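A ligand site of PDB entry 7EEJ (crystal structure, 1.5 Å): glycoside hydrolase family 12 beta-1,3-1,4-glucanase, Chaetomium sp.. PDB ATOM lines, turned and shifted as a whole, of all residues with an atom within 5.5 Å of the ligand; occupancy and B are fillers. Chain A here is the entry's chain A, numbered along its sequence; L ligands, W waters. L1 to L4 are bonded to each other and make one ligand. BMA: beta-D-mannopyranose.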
ATOM      1  N   TYR A  13      25.960 -24.759   1.031  1.00  0.00           N
ATOM      2  CA  TYR A  13      24.553 -25.108   1.231  1.00  0.00           C
ATOM      3  C   TYR A  13      24.250 -25.572   2.643  1.00  0.00           C
ATOM      4  O   TYR A  13      23.211 -26.195   2.879  1.00  0.00           O
ATOM      5  CB  TYR A  13      24.016 -26.092   0.176  1.00  0.00           C
ATOM      6  CG  TYR A  13      24.370 -25.712  -1.234  1.00  0.00           C
ATOM      7  CD1 TYR A  13      24.230 -24.407  -1.696  1.00  0.00           C
ATOM      8  CD2 TYR A  13      24.878 -26.667  -2.120  1.00  0.00           C
ATOM      9  CE1 TYR A  13      24.571 -24.067  -2.990  1.00  0.00           C
ATOM     10  CE2 TYR A  13      25.218 -26.341  -3.414  1.00  0.00           C
ATOM     11  CZ  TYR A  13      25.059 -25.048  -3.852  1.00  0.00           C
ATOM     12  OH  TYR A  13      25.400 -24.743  -5.152  1.00  0.00           O
ATOM     13  N   TYR A  15      22.649 -25.451   6.151  1.00  0.00           N
ATOM     14  CA  TYR A  15      21.244 -25.069   6.244  1.00  0.00           C
ATOM     15  C   TYR A  15      20.762 -25.107   7.690  1.00  0.00           C
ATOM     16  O   TYR A  15      21.073 -26.029   8.448  1.00  0.00           O
ATOM     17  CB  TYR A  15      20.399 -26.003   5.365  1.00  0.00           C
ATOM     18  CG  TYR A  15      18.914 -25.720   5.384  1.00  0.00           C
ATOM     19  CD1 TYR A  15      18.371 -24.709   4.600  1.00  0.00           C
ATOM     20  CD2 TYR A  15      18.048 -26.478   6.165  1.00  0.00           C
ATOM     21  CE1 TYR A  15      17.007 -24.453   4.603  1.00  0.00           C
ATOM     22  CE2 TYR A  15      16.674 -26.235   6.180  1.00  0.00           C
ATOM     23  CZ  TYR A  15      16.168 -25.221   5.379  1.00  0.00           C
ATOM     24  OH  TYR A  15      14.810 -24.980   5.405  1.00  0.00           O
ATOM     25  N   GLU A  22      14.675 -19.619   7.708  1.00  0.00           N
ATOM     26  CA  GLU A  22      15.759 -20.517   7.387  1.00  0.00           C
ATOM     27  C   GLU A  22      16.963 -19.671   7.006  1.00  0.00           C
ATOM     28  O   GLU A  22      16.820 -18.499   6.633  1.00  0.00           O
ATOM     29  CB  GLU A  22      15.393 -21.485   6.252  1.00  0.00           C
ATOM     30  CG  GLU A  22      15.033 -20.798   4.931  1.00  0.00           C
ATOM     31  CD  GLU A  22      14.619 -21.782   3.859  1.00  0.00           C
ATOM     32  OE1 GLU A  22      13.963 -22.802   4.177  1.00  0.00           O
ATOM     33  OE2 GLU A  22      14.953 -21.533   2.681  1.00  0.00           O
ATOM     34  N   ASN A  24      20.622 -20.260   4.595  1.00  0.00           N
ATOM     35  CA  ASN A  24      21.373 -21.134   3.710  1.00  0.00           C
ATOM     36  C   ASN A  24      22.705 -20.472   3.402  1.00  0.00           C
ATOM     37  O   ASN A  24      22.737 -19.365   2.846  1.00  0.00           O
ATOM     38  CB  ASN A  24      20.586 -21.425   2.431  1.00  0.00           C
ATOM     39  CG  ASN A  24      21.208 -22.533   1.607  1.00  0.00           C
ATOM     40  OD1 ASN A  24      22.374 -22.458   1.223  1.00  0.00           O
ATOM     41  ND2 ASN A  24      20.420 -23.567   1.318  1.00  0.00           N
ATOM     42  N   ASN A  26      24.734 -20.221   1.065  1.00  0.00           N
ATOM     43  CA  ASN A  26      24.452 -20.554  -0.336  1.00  0.00           C
ATOM     44  C   ASN A  26      25.620 -20.130  -1.238  1.00  0.00           C
ATOM     45  O   ASN A  26      25.570 -19.151  -1.989  1.00  0.00           O
ATOM     46  CB  ASN A  26      23.137 -19.881  -0.719  1.00  0.00           C
ATOM     47  CG  ASN A  26      22.803 -19.989  -2.187  1.00  0.00           C
ATOM     48  OD1 ASN A  26      23.106 -20.989  -2.848  1.00  0.00           O
ATOM     49  ND2 ASN A  26      22.143 -18.962  -2.706  1.00  0.00           N
ATOM     50  N   TRP A  28      26.851 -20.799  -4.038  1.00  0.00           N
ATOM     51  CA  TRP A  28      26.554 -21.485  -5.297  1.00  0.00           C
ATOM     52  C   TRP A  28      27.611 -21.228  -6.377  1.00  0.00           C
ATOM     53  O   TRP A  28      27.779 -22.060  -7.272  1.00  0.00           O
ATOM     54  CB  TRP A  28      25.154 -21.110  -5.792  1.00  0.00           C
ATOM     55  CG  TRP A  28      24.978 -19.672  -6.168  1.00  0.00           C
ATOM     56  CD1 TRP A  28      24.483 -18.678  -5.381  1.00  0.00           C
ATOM     57  CD2 TRP A  28      25.276 -19.078  -7.437  1.00  0.00           C
ATOM     58  NE1 TRP A  28      24.467 -17.495  -6.083  1.00  0.00           N
ATOM     59  CE2 TRP A  28      24.944 -17.711  -7.352  1.00  0.00           C
ATOM     60  CE3 TRP A  28      25.802 -19.561  -8.640  1.00  0.00           C
ATOM     61  CZ2 TRP A  28      25.116 -16.830  -8.406  1.00  0.00           C
ATOM     62  CZ3 TRP A  28      25.974 -18.681  -9.694  1.00  0.00           C
ATOM     63  CH2 TRP A  28      25.635 -17.334  -9.568  1.00  0.00           C
ATOM     64  N   VAL A  65      29.338 -13.815  -9.262  1.00  0.00           N
ATOM     65  CA  VAL A  65      28.871 -13.991  -7.889  1.00  0.00           C
ATOM     66  C   VAL A  65      29.421 -15.297  -7.344  1.00  0.00           C
ATOM     67  O   VAL A  65      29.303 -16.358  -7.979  1.00  0.00           O
ATOM     68  CB  VAL A  65      27.329 -14.000  -7.867  1.00  0.00           C
ATOM     69  CG1 VAL A  65      26.805 -14.397  -6.481  1.00  0.00           C
ATOM     70  CG2 VAL A  65      26.807 -12.653  -8.291  1.00  0.00           C
ATOM     71  N   SER A  67      28.507 -16.279  -4.083  1.00  0.00           N
ATOM     72  CA  SER A  67      27.571 -16.756  -3.081  1.00  0.00           C
ATOM     73  C   SER A  67      26.449 -15.736  -2.946  1.00  0.00           C
ATOM     74  O   SER A  67      26.630 -14.550  -3.253  1.00  0.00           O
ATOM     75  CB  SER A  67      28.273 -16.903  -1.728  1.00  0.00           C
ATOM     76  OG  SER A  67      28.730 -15.646  -1.259  1.00  0.00           O
ATOM     77  N   TYR A  68      25.302 -16.224  -2.476  1.00  0.00           N
ATOM     78  CA  TYR A  68      24.200 -15.373  -2.033  1.00  0.00           C
ATOM     79  C   TYR A  68      23.678 -16.057  -0.776  1.00  0.00           C
ATOM     80  O   TYR A  68      22.639 -16.733  -0.771  1.00  0.00           O
ATOM     81  CB  TYR A  68      23.118 -15.224  -3.100  1.00  0.00           C
ATOM     82  CG  TYR A  68      21.884 -14.515  -2.617  1.00  0.00           C
ATOM     83  CD1 TYR A  68      21.931 -13.186  -2.205  1.00  0.00           C
ATOM     84  CD2 TYR A  68      20.650 -15.169  -2.544  1.00  0.00           C
ATOM     85  CE1 TYR A  68      20.788 -12.522  -1.748  1.00  0.00           C
ATOM     86  CE2 TYR A  68      19.499 -14.505  -2.094  1.00  0.00           C
ATOM     87  CZ  TYR A  68      19.581 -13.186  -1.681  1.00  0.00           C
ATOM     88  OH  TYR A  68      18.457 -12.532  -1.219  1.00  0.00           O
ATOM     89  N   TYR A  70      21.704 -16.282   2.565  1.00  0.00           N
ATOM     90  CA  TYR A  70      20.437 -15.600   2.800  1.00  0.00           C
ATOM     91  C   TYR A  70      19.720 -16.156   4.019  1.00  0.00           C
ATOM     92  O   TYR A  70      19.958 -17.294   4.439  1.00  0.00           O
ATOM     93  CB  TYR A  70      19.492 -15.709   1.593  1.00  0.00           C
ATOM     94  CG  TYR A  70      19.132 -17.133   1.174  1.00  0.00           C
ATOM     95  CD1 TYR A  70      18.167 -17.859   1.873  1.00  0.00           C
ATOM     96  CD2 TYR A  70      19.723 -17.714   0.054  1.00  0.00           C
ATOM     97  CE1 TYR A  70      17.824 -19.149   1.481  1.00  0.00           C
ATOM     98  CE2 TYR A  70      19.378 -18.997  -0.350  1.00  0.00           C
ATOM     99  CZ  TYR A  70      18.431 -19.711   0.361  1.00  0.00           C
ATOM    100  OH  TYR A  70      18.095 -20.981  -0.037  1.00  0.00           O
ATOM    101  N   ASP A 107      15.787 -11.425  -2.732  1.00  0.00           N
ATOM    102  CA  ASP A 107      15.653 -12.270  -3.913  1.00  0.00           C
ATOM    103  C   ASP A 107      14.344 -13.036  -3.805  1.00  0.00           C
ATOM    104  O   ASP A 107      14.077 -13.700  -2.794  1.00  0.00           O
ATOM    105  CB  ASP A 107      16.826 -13.267  -4.030  1.00  0.00           C
ATOM    106  CG  ASP A 107      17.028 -13.767  -5.454  1.00  0.00           C
ATOM    107  OD1 ASP A 107      16.612 -13.063  -6.390  1.00  0.00           O
ATOM    108  OD2 ASP A 107      17.596 -14.862  -5.639  1.00  0.00           O
ATOM    109  N   PHE A 109      11.763 -15.562  -6.256  1.00  0.00           N
ATOM    110  CA  PHE A 109      11.470 -16.291  -7.491  1.00  0.00           C
ATOM    111  C   PHE A 109       9.979 -16.555  -7.541  1.00  0.00           C
ATOM    112  O   PHE A 109       9.365 -16.868  -6.514  1.00  0.00           O
ATOM    113  CB  PHE A 109      12.173 -17.641  -7.539  1.00  0.00           C
ATOM    114  CG  PHE A 109      13.665 -17.571  -7.706  1.00  0.00           C
ATOM    115  CD1 PHE A 109      14.246 -16.727  -8.647  1.00  0.00           C
ATOM    116  CD2 PHE A 109      14.497 -18.379  -6.933  1.00  0.00           C
ATOM    117  CE1 PHE A 109      15.641 -16.682  -8.786  1.00  0.00           C
ATOM    118  CE2 PHE A 109      15.871 -18.339  -7.079  1.00  0.00           C
ATOM    119  CZ  PHE A 109      16.441 -17.486  -8.002  1.00  0.00           C
ATOM    120  N   ASN A 118      13.563 -24.526  -5.939  1.00  0.00           N
ATOM    121  CA  ASN A 118      13.771 -23.233  -5.277  1.00  0.00           C
ATOM    122  C   ASN A 118      14.975 -22.452  -5.802  1.00  0.00           C
ATOM    123  O   ASN A 118      15.201 -21.320  -5.357  1.00  0.00           O
ATOM    124  CB  ASN A 118      13.858 -23.439  -3.767  1.00  0.00           C
ATOM    125  CG  ASN A 118      15.252 -23.836  -3.318  1.00  0.00           C
ATOM    126  OD1 ASN A 118      16.000 -24.459  -4.061  1.00  0.00           O
ATOM    127  ND2 ASN A 118      15.587 -23.482  -2.089  1.00  0.00           N
ATOM    128  N   SER A 119      15.734 -22.994  -6.753  1.00  0.00           N
ATOM    129  CA  SER A 119      16.968 -22.373  -7.224  1.00  0.00           C
ATOM    130  C   SER A 119      16.762 -21.424  -8.398  1.00  0.00           C
ATOM    131  O   SER A 119      17.732 -20.780  -8.824  1.00  0.00           O
ATOM    132  CB  SER A 119      17.979 -23.455  -7.607  1.00  0.00           C
ATOM    133  OG  SER A 119      17.359 -24.463  -8.397  1.00  0.00           O
ATOM    134  N   SER A 120      15.553 -21.340  -8.940  1.00  0.00           N
ATOM    135  CA  SER A 120      15.238 -20.407 -10.016  1.00  0.00           C
ATOM    136  C   SER A 120      13.724 -20.321 -10.104  1.00  0.00           C
ATOM    137  O   SER A 120      13.003 -20.916  -9.295  1.00  0.00           O
ATOM    138  CB  SER A 120      15.860 -20.845 -11.345  1.00  0.00           C
ATOM    139  OG  SER A 120      15.371 -22.119 -11.704  1.00  0.00           O
ATOM    140  N   GLU A 124      12.322 -13.513 -11.715  1.00  0.00           N
ATOM    141  CA  GLU A 124      13.057 -13.189 -10.511  1.00  0.00           C
ATOM    142  C   GLU A 124      12.891 -11.709 -10.213  1.00  0.00           C
ATOM    143  O   GLU A 124      12.971 -10.867 -11.111  1.00  0.00           O
ATOM    144  CB  GLU A 124      14.541 -13.488 -10.686  1.00  0.00           C
ATOM    145  CG  GLU A 124      15.347 -13.186  -9.465  1.00  0.00           C
ATOM    146  CD  GLU A 124      16.790 -13.566  -9.627  1.00  0.00           C
ATOM    147  OE1 GLU A 124      17.206 -13.837 -10.770  1.00  0.00           O
ATOM    148  OE2 GLU A 124      17.500 -13.589  -8.611  1.00  0.00           O
ATOM    149  N   MET A 126      14.574  -8.899  -7.697  1.00  0.00           N
ATOM    150  CA  MET A 126      15.589  -8.544  -6.723  1.00  0.00           C
ATOM    151  C   MET A 126      15.372  -7.107  -6.291  1.00  0.00           C
ATOM    152  O   MET A 126      14.997  -6.250  -7.090  1.00  0.00           O
ATOM    153  CB  MET A 126      17.003  -8.662  -7.304  1.00  0.00           C
ATOM    154  CG  MET A 126      17.319 -10.027  -7.898  1.00  0.00           C
ATOM    155  SD  MET A 126      19.097 -10.166  -8.113  1.00  0.00           S
ATOM    156  CE  MET A 126      19.573 -10.591  -6.435  1.00  0.00           C
ATOM    157  N   ILE A 138      21.776  -7.984 -13.452  1.00  0.00           N
ATOM    158  CA  ILE A 138      21.500  -8.594 -14.746  1.00  0.00           C
ATOM    159  C   ILE A 138      20.808  -7.597 -15.670  1.00  0.00           C
ATOM    160  O   ILE A 138      19.922  -6.834 -15.247  1.00  0.00           O
ATOM    161  CB  ILE A 138      20.641  -9.857 -14.559  1.00  0.00           C
ATOM    162  CG1 ILE A 138      21.523 -10.986 -14.019  1.00  0.00           C
ATOM    163  CG2 ILE A 138      19.945 -10.250 -15.842  1.00  0.00           C
ATOM    164  CD1 ILE A 138      20.739 -12.103 -13.435  1.00  0.00           C
ATOM    165  N   ASN A 159      18.313 -14.216 -17.477  1.00  0.00           N
ATOM    166  CA  ASN A 159      19.285 -15.199 -17.007  1.00  0.00           C
ATOM    167  C   ASN A 159      18.788 -16.523 -17.550  1.00  0.00           C
ATOM    168  O   ASN A 159      17.913 -17.154 -16.944  1.00  0.00           O
ATOM    169  CB  ASN A 159      19.370 -15.192 -15.482  1.00  0.00           C
ATOM    170  CG  ASN A 159      20.391 -16.179 -14.943  1.00  0.00           C
ATOM    171  OD1 ASN A 159      20.940 -17.001 -15.679  1.00  0.00           O
ATOM    172  ND2 ASN A 159      20.654 -16.101 -13.637  1.00  0.00           N
ATOM    173  N   MET A 162      14.950 -17.194 -17.632  1.00  0.00           N
ATOM    174  CA  MET A 162      14.332 -16.516 -16.496  1.00  0.00           C
ATOM    175  C   MET A 162      14.490 -14.999 -16.656  1.00  0.00           C
ATOM    176  O   MET A 162      15.609 -14.519 -16.884  1.00  0.00           O
ATOM    177  CB  MET A 162      14.984 -16.971 -15.186  1.00  0.00           C
ATOM    178  CG  MET A 162      14.491 -16.228 -13.957  1.00  0.00           C
ATOM    179  SD  MET A 162      15.094 -16.925 -12.408  1.00  0.00           S
ATOM    180  CE  MET A 162      16.846 -16.655 -12.547  1.00  0.00           C
ATOM    181  N   VAL A 164      14.604 -11.303 -15.152  1.00  0.00           N
ATOM    182  CA  VAL A 164      15.089 -10.780 -13.884  1.00  0.00           C
ATOM    183  C   VAL A 164      14.821  -9.278 -13.834  1.00  0.00           C
ATOM    184  O   VAL A 164      15.305  -8.529 -14.688  1.00  0.00           O
ATOM    185  CB  VAL A 164      16.589 -11.049 -13.701  1.00  0.00           C
ATOM    186  CG1 VAL A 164      17.075 -10.546 -12.334  1.00  0.00           C
ATOM    187  CG2 VAL A 164      16.866 -12.518 -13.895  1.00  0.00           C
ATOM    188  N   GLN A 204      13.624 -14.146   0.042  1.00  0.00           N
ATOM    189  CA  GLN A 204      14.915 -14.223   0.712  1.00  0.00           C
ATOM    190  C   GLN A 204      15.541 -12.839   0.845  1.00  0.00           C
ATOM    191  O   GLN A 204      15.297 -11.946   0.042  1.00  0.00           O
ATOM    192  CB  GLN A 204      15.884 -15.120  -0.066  1.00  0.00           C
ATOM    193  CG  GLN A 204      15.400 -16.562  -0.215  1.00  0.00           C
ATOM    194  CD  GLN A 204      16.130 -17.301  -1.309  1.00  0.00           C
ATOM    195  OE1 GLN A 204      16.847 -16.713  -2.130  1.00  0.00           O
ATOM    196  NE2 GLN A 204      15.946 -18.619  -1.341  1.00  0.00           N
ATOM    197  N   GLU A 208      24.888 -10.776  -2.151  1.00  0.00           N
ATOM    198  CA  GLU A 208      25.661 -11.385  -3.235  1.00  0.00           C
ATOM    199  C   GLU A 208      27.112 -10.909  -3.101  1.00  0.00           C
ATOM    200  O   GLU A 208      27.383  -9.716  -3.223  1.00  0.00           O
ATOM    201  CB  GLU A 208      25.107 -10.976  -4.601  1.00  0.00           C
ATOM    202  CG  GLU A 208      23.747 -11.571  -4.928  1.00  0.00           C
ATOM    203  CD  GLU A 208      23.369 -11.404  -6.400  1.00  0.00           C
ATOM    204  OE1 GLU A 208      23.102 -10.269  -6.831  1.00  0.00           O
ATOM    205  OE2 GLU A 208      23.352 -12.413  -7.133  1.00  0.00           O
HETATM  206  C1  BMA L   1      20.297 -13.602  -9.188  1.00  0.00           C
HETATM  207  C2  BMA L   1      19.841 -14.807 -10.079  1.00  0.00           C
HETATM  208  C3  BMA L   1      19.991 -16.240  -9.495  1.00  0.00           C
HETATM  209  C4  BMA L   1      20.846 -16.312  -8.205  1.00  0.00           C
HETATM  210  C5  BMA L   1      20.620 -15.034  -7.373  1.00  0.00           C
HETATM  211  C6  BMA L   1      21.381 -15.032  -6.096  1.00  0.00           C
HETATM  212  O1  BMA L   1      20.947 -12.651 -10.037  1.00  0.00           O
HETATM  213  O2  BMA L   1      20.351 -14.728 -11.386  1.00  0.00           O
HETATM  214  O3  BMA L   1      20.437 -17.174 -10.479  1.00  0.00           O
HETATM  215  O4  BMA L   1      20.162 -17.290  -7.518  1.00  0.00           O
HETATM  216  O5  BMA L   1      21.124 -13.945  -8.138  1.00  0.00           O
HETATM  217  O6  BMA L   1      22.772 -14.995  -6.420  1.00  0.00           O
HETATM  218  C1  BMA L   2      21.191 -18.276  -7.399  1.00  0.00           C
HETATM  219  C2  BMA L   2      21.121 -19.057  -5.993  1.00  0.00           C
HETATM  220  C3  BMA L   2      20.997 -20.652  -6.080  1.00  0.00           C
HETATM  221  C4  BMA L   2      21.150 -21.218  -7.498  1.00  0.00           C
HETATM  222  C5  BMA L   2      21.978 -20.250  -8.334  1.00  0.00           C
HETATM  223  C6  BMA L   2      22.372 -20.784  -9.687  1.00  0.00           C
HETATM  224  O2  BMA L   2      20.218 -18.521  -5.066  1.00  0.00           O
HETATM  225  O3  BMA L   2      19.905 -21.300  -5.348  1.00  0.00           O
HETATM  226  O4  BMA L   2      21.838 -22.430  -7.403  1.00  0.00           O
HETATM  227  O5  BMA L   2      21.173 -19.104  -8.533  1.00  0.00           O
HETATM  228  O6  BMA L   2      21.201 -21.190 -10.368  1.00  0.00           O
HETATM  229  C1  BMA L   3      20.578 -22.203  -4.419  1.00  0.00           C
HETATM  230  C2  BMA L   3      19.907 -22.163  -2.924  1.00  0.00           C
HETATM  231  C3  BMA L   3      19.735 -23.566  -2.199  1.00  0.00           C
HETATM  232  C4  BMA L   3      20.124 -24.813  -3.029  1.00  0.00           C
HETATM  233  C5  BMA L   3      21.238 -24.440  -4.001  1.00  0.00           C
HETATM  234  C6  BMA L   3      21.835 -25.616  -4.732  1.00  0.00           C
HETATM  235  O2  BMA L   3      18.720 -21.399  -2.804  1.00  0.00           O
HETATM  236  O3  BMA L   3      18.440 -23.717  -1.613  1.00  0.00           O
HETATM  237  O4  BMA L   3      20.684 -25.704  -2.131  1.00  0.00           O
HETATM  238  O5  BMA L   3      20.630 -23.544  -4.934  1.00  0.00           O
HETATM  239  O6  BMA L   3      20.784 -26.347  -5.333  1.00  0.00           O
HETATM  240  C1  BMA L   4      19.790 -26.660  -1.578  1.00  0.00           C
HETATM  241  C2  BMA L   4      20.510 -28.067  -1.469  1.00  0.00           C
HETATM  242  C3  BMA L   4      19.969 -28.970  -0.303  1.00  0.00           C
HETATM  243  C4  BMA L   4      19.269 -28.213   0.855  1.00  0.00           C
HETATM  244  C5  BMA L   4      18.427 -27.053   0.297  1.00  0.00           C
HETATM  245  C6  BMA L   4      17.663 -26.289   1.356  1.00  0.00           C
HETATM  246  O2  BMA L   4      21.905 -27.955  -1.309  1.00  0.00           O
HETATM  247  O3  BMA L   4      21.010 -29.775   0.218  1.00  0.00           O
HETATM  248  O4  BMA L   4      18.413 -29.100   1.586  1.00  0.00           O
HETATM  249  O5  BMA L   4      19.343 -26.164  -0.347  1.00  0.00           O
HETATM  250  O6  BMA L   4      16.743 -25.406   0.680  1.00  0.00           O
HETATM  251  O   HOH W   1      23.793 -12.886 -10.202  1.00  0.00           O
HETATM  252  O   HOH W   2      18.080 -17.250  -4.521  1.00  0.00           O
HETATM  253  O   HOH W   3      18.988 -19.409 -10.724  1.00  0.00           O
HETATM  254  O   HOH W   4      19.795 -18.281 -12.740  1.00  0.00           O
HETATM  255  O   HOH W   5      16.159 -26.151  -1.712  1.00  0.00           O
HETATM  256  O   HOH W   6      21.728 -19.754 -12.996  1.00  0.00           O
HETATM  257  O   HOH W   7      17.039 -19.820  -3.974  1.00  0.00           O
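Merely in contact with the ligand: Tyr 13, Tyr 68, Ile 138, Asp 107, Ser 119, Tyr 15 and Phe 109. Hydrophobic or aromatic side chains within 4 Å of the ligand: Tyr 13, Tyr 15, Trp 28, Tyr 68, Tyr 70, Phe 109, Met 126 and Ile 138. Within 4 Å of the ligand: Tyr 13, Tyr 15, Asn 24, Asn 26, Trp 28, Tyr 68, Tyr 70, Asp 107, Phe 109, Asn 118, Ser 119, Glu 124, Met 126, Ile 138, Asn 159 and Glu 208.
An oxygen (O2) of BMA L1 sits close to the side-chain carboxylate (OE1) of Glu 124, at 3.3 Å. ND2 of Asn 159 lies within hydrogen-bond range of O2 of BMA L1, 2.7 Å away. An oxygen (O6) of BMA L1 sits at hydrogen-bond distance from the side-chain carboxylate (OE2) of Glu 208, 2.7 Å away. An oxygen (O5) of BMA L4 sits at hydrogen-bond distance from the side-chain amide nitrogen (ND2) of Asn 24 (3.3 Å). An oxygen (O3) of BMA L3 sits at hydrogen-bond distance from the side-chain amide nitrogen (ND2) of Asn 118 (2.9 Å). NE1 of Trp 28 is in hydrogen-bond range of O6 of BMA L1 (3.0 Å). The side-chain sulfur (SD) of Met 126 is in hydrogen-bond range of an oxygen (O1) of BMA L1, at 3.6 Å. ND2 of Asn 26 lies within hydrogen-bond range of O2 of BMA L2. OH of Tyr 70 is in hydrogen-bond range of O2 of BMA L3 (2.9 Å).
Water W2 lies within hydrogen-bond range of O2 of BMA L2 (2.5 Å), OD2 of Asp 107 (2.7 Å) and OE1 of Gln 204 (2.7 Å). Water W5 lies within hydrogen-bond range of O6 of BMA L4 (2.6 Å) and ND2 of Asn 118 (2.8 Å). Water W7 lies within hydrogen-bond range of an oxygen (O2) of BMA L3, the backbone carbonyl oxygen of Asn 118 and the side-chain amide nitrogen of Gln 204. Water W4 bridges the side-chain amide nitrogen (ND2) of Asn 159 (2.5 Å) and an oxygen (O3) of BMA L1 (2.6 Å). Water W3 bridges the backbone carbonyl oxygen (O) of Ser 119 and an oxygen (O3) of BMA L1. Water W1 bridges an oxygen (O1) of BMA L1 and the side-chain carboxylate (OE2) of Glu 208.
The side-chain hydroxyl of Tyr 15 sits at hydrogen-bond distance from the side-chain carboxylate of Glu 22, 2.6 Å away. The backbone NH (N) of Tyr 68 is in hydrogen-bond range of the backbone carbonyl oxygen (O) of Asn 26 (3.0 Å). N of Asn 26 sits close to OD1 of Asn 24. O of Tyr 70 lies within hydrogen-bond range of N of Asn 24 (3.0 Å). OH of Tyr 68 sits at hydrogen-bond distance from O of Gln 204. The backbone NH (N) of Asp 107 lies within hydrogen-bond range of the backbone carbonyl oxygen (O) of Gln 204 (2.9 Å). OH of Tyr 68 is in hydrogen-bond range of N of Asp 107, at 3.3 Å. The side-chain amide nitrogen (NE2) of Gln 204 lies close to the side-chain hydroxyl (OH) of Tyr 70.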
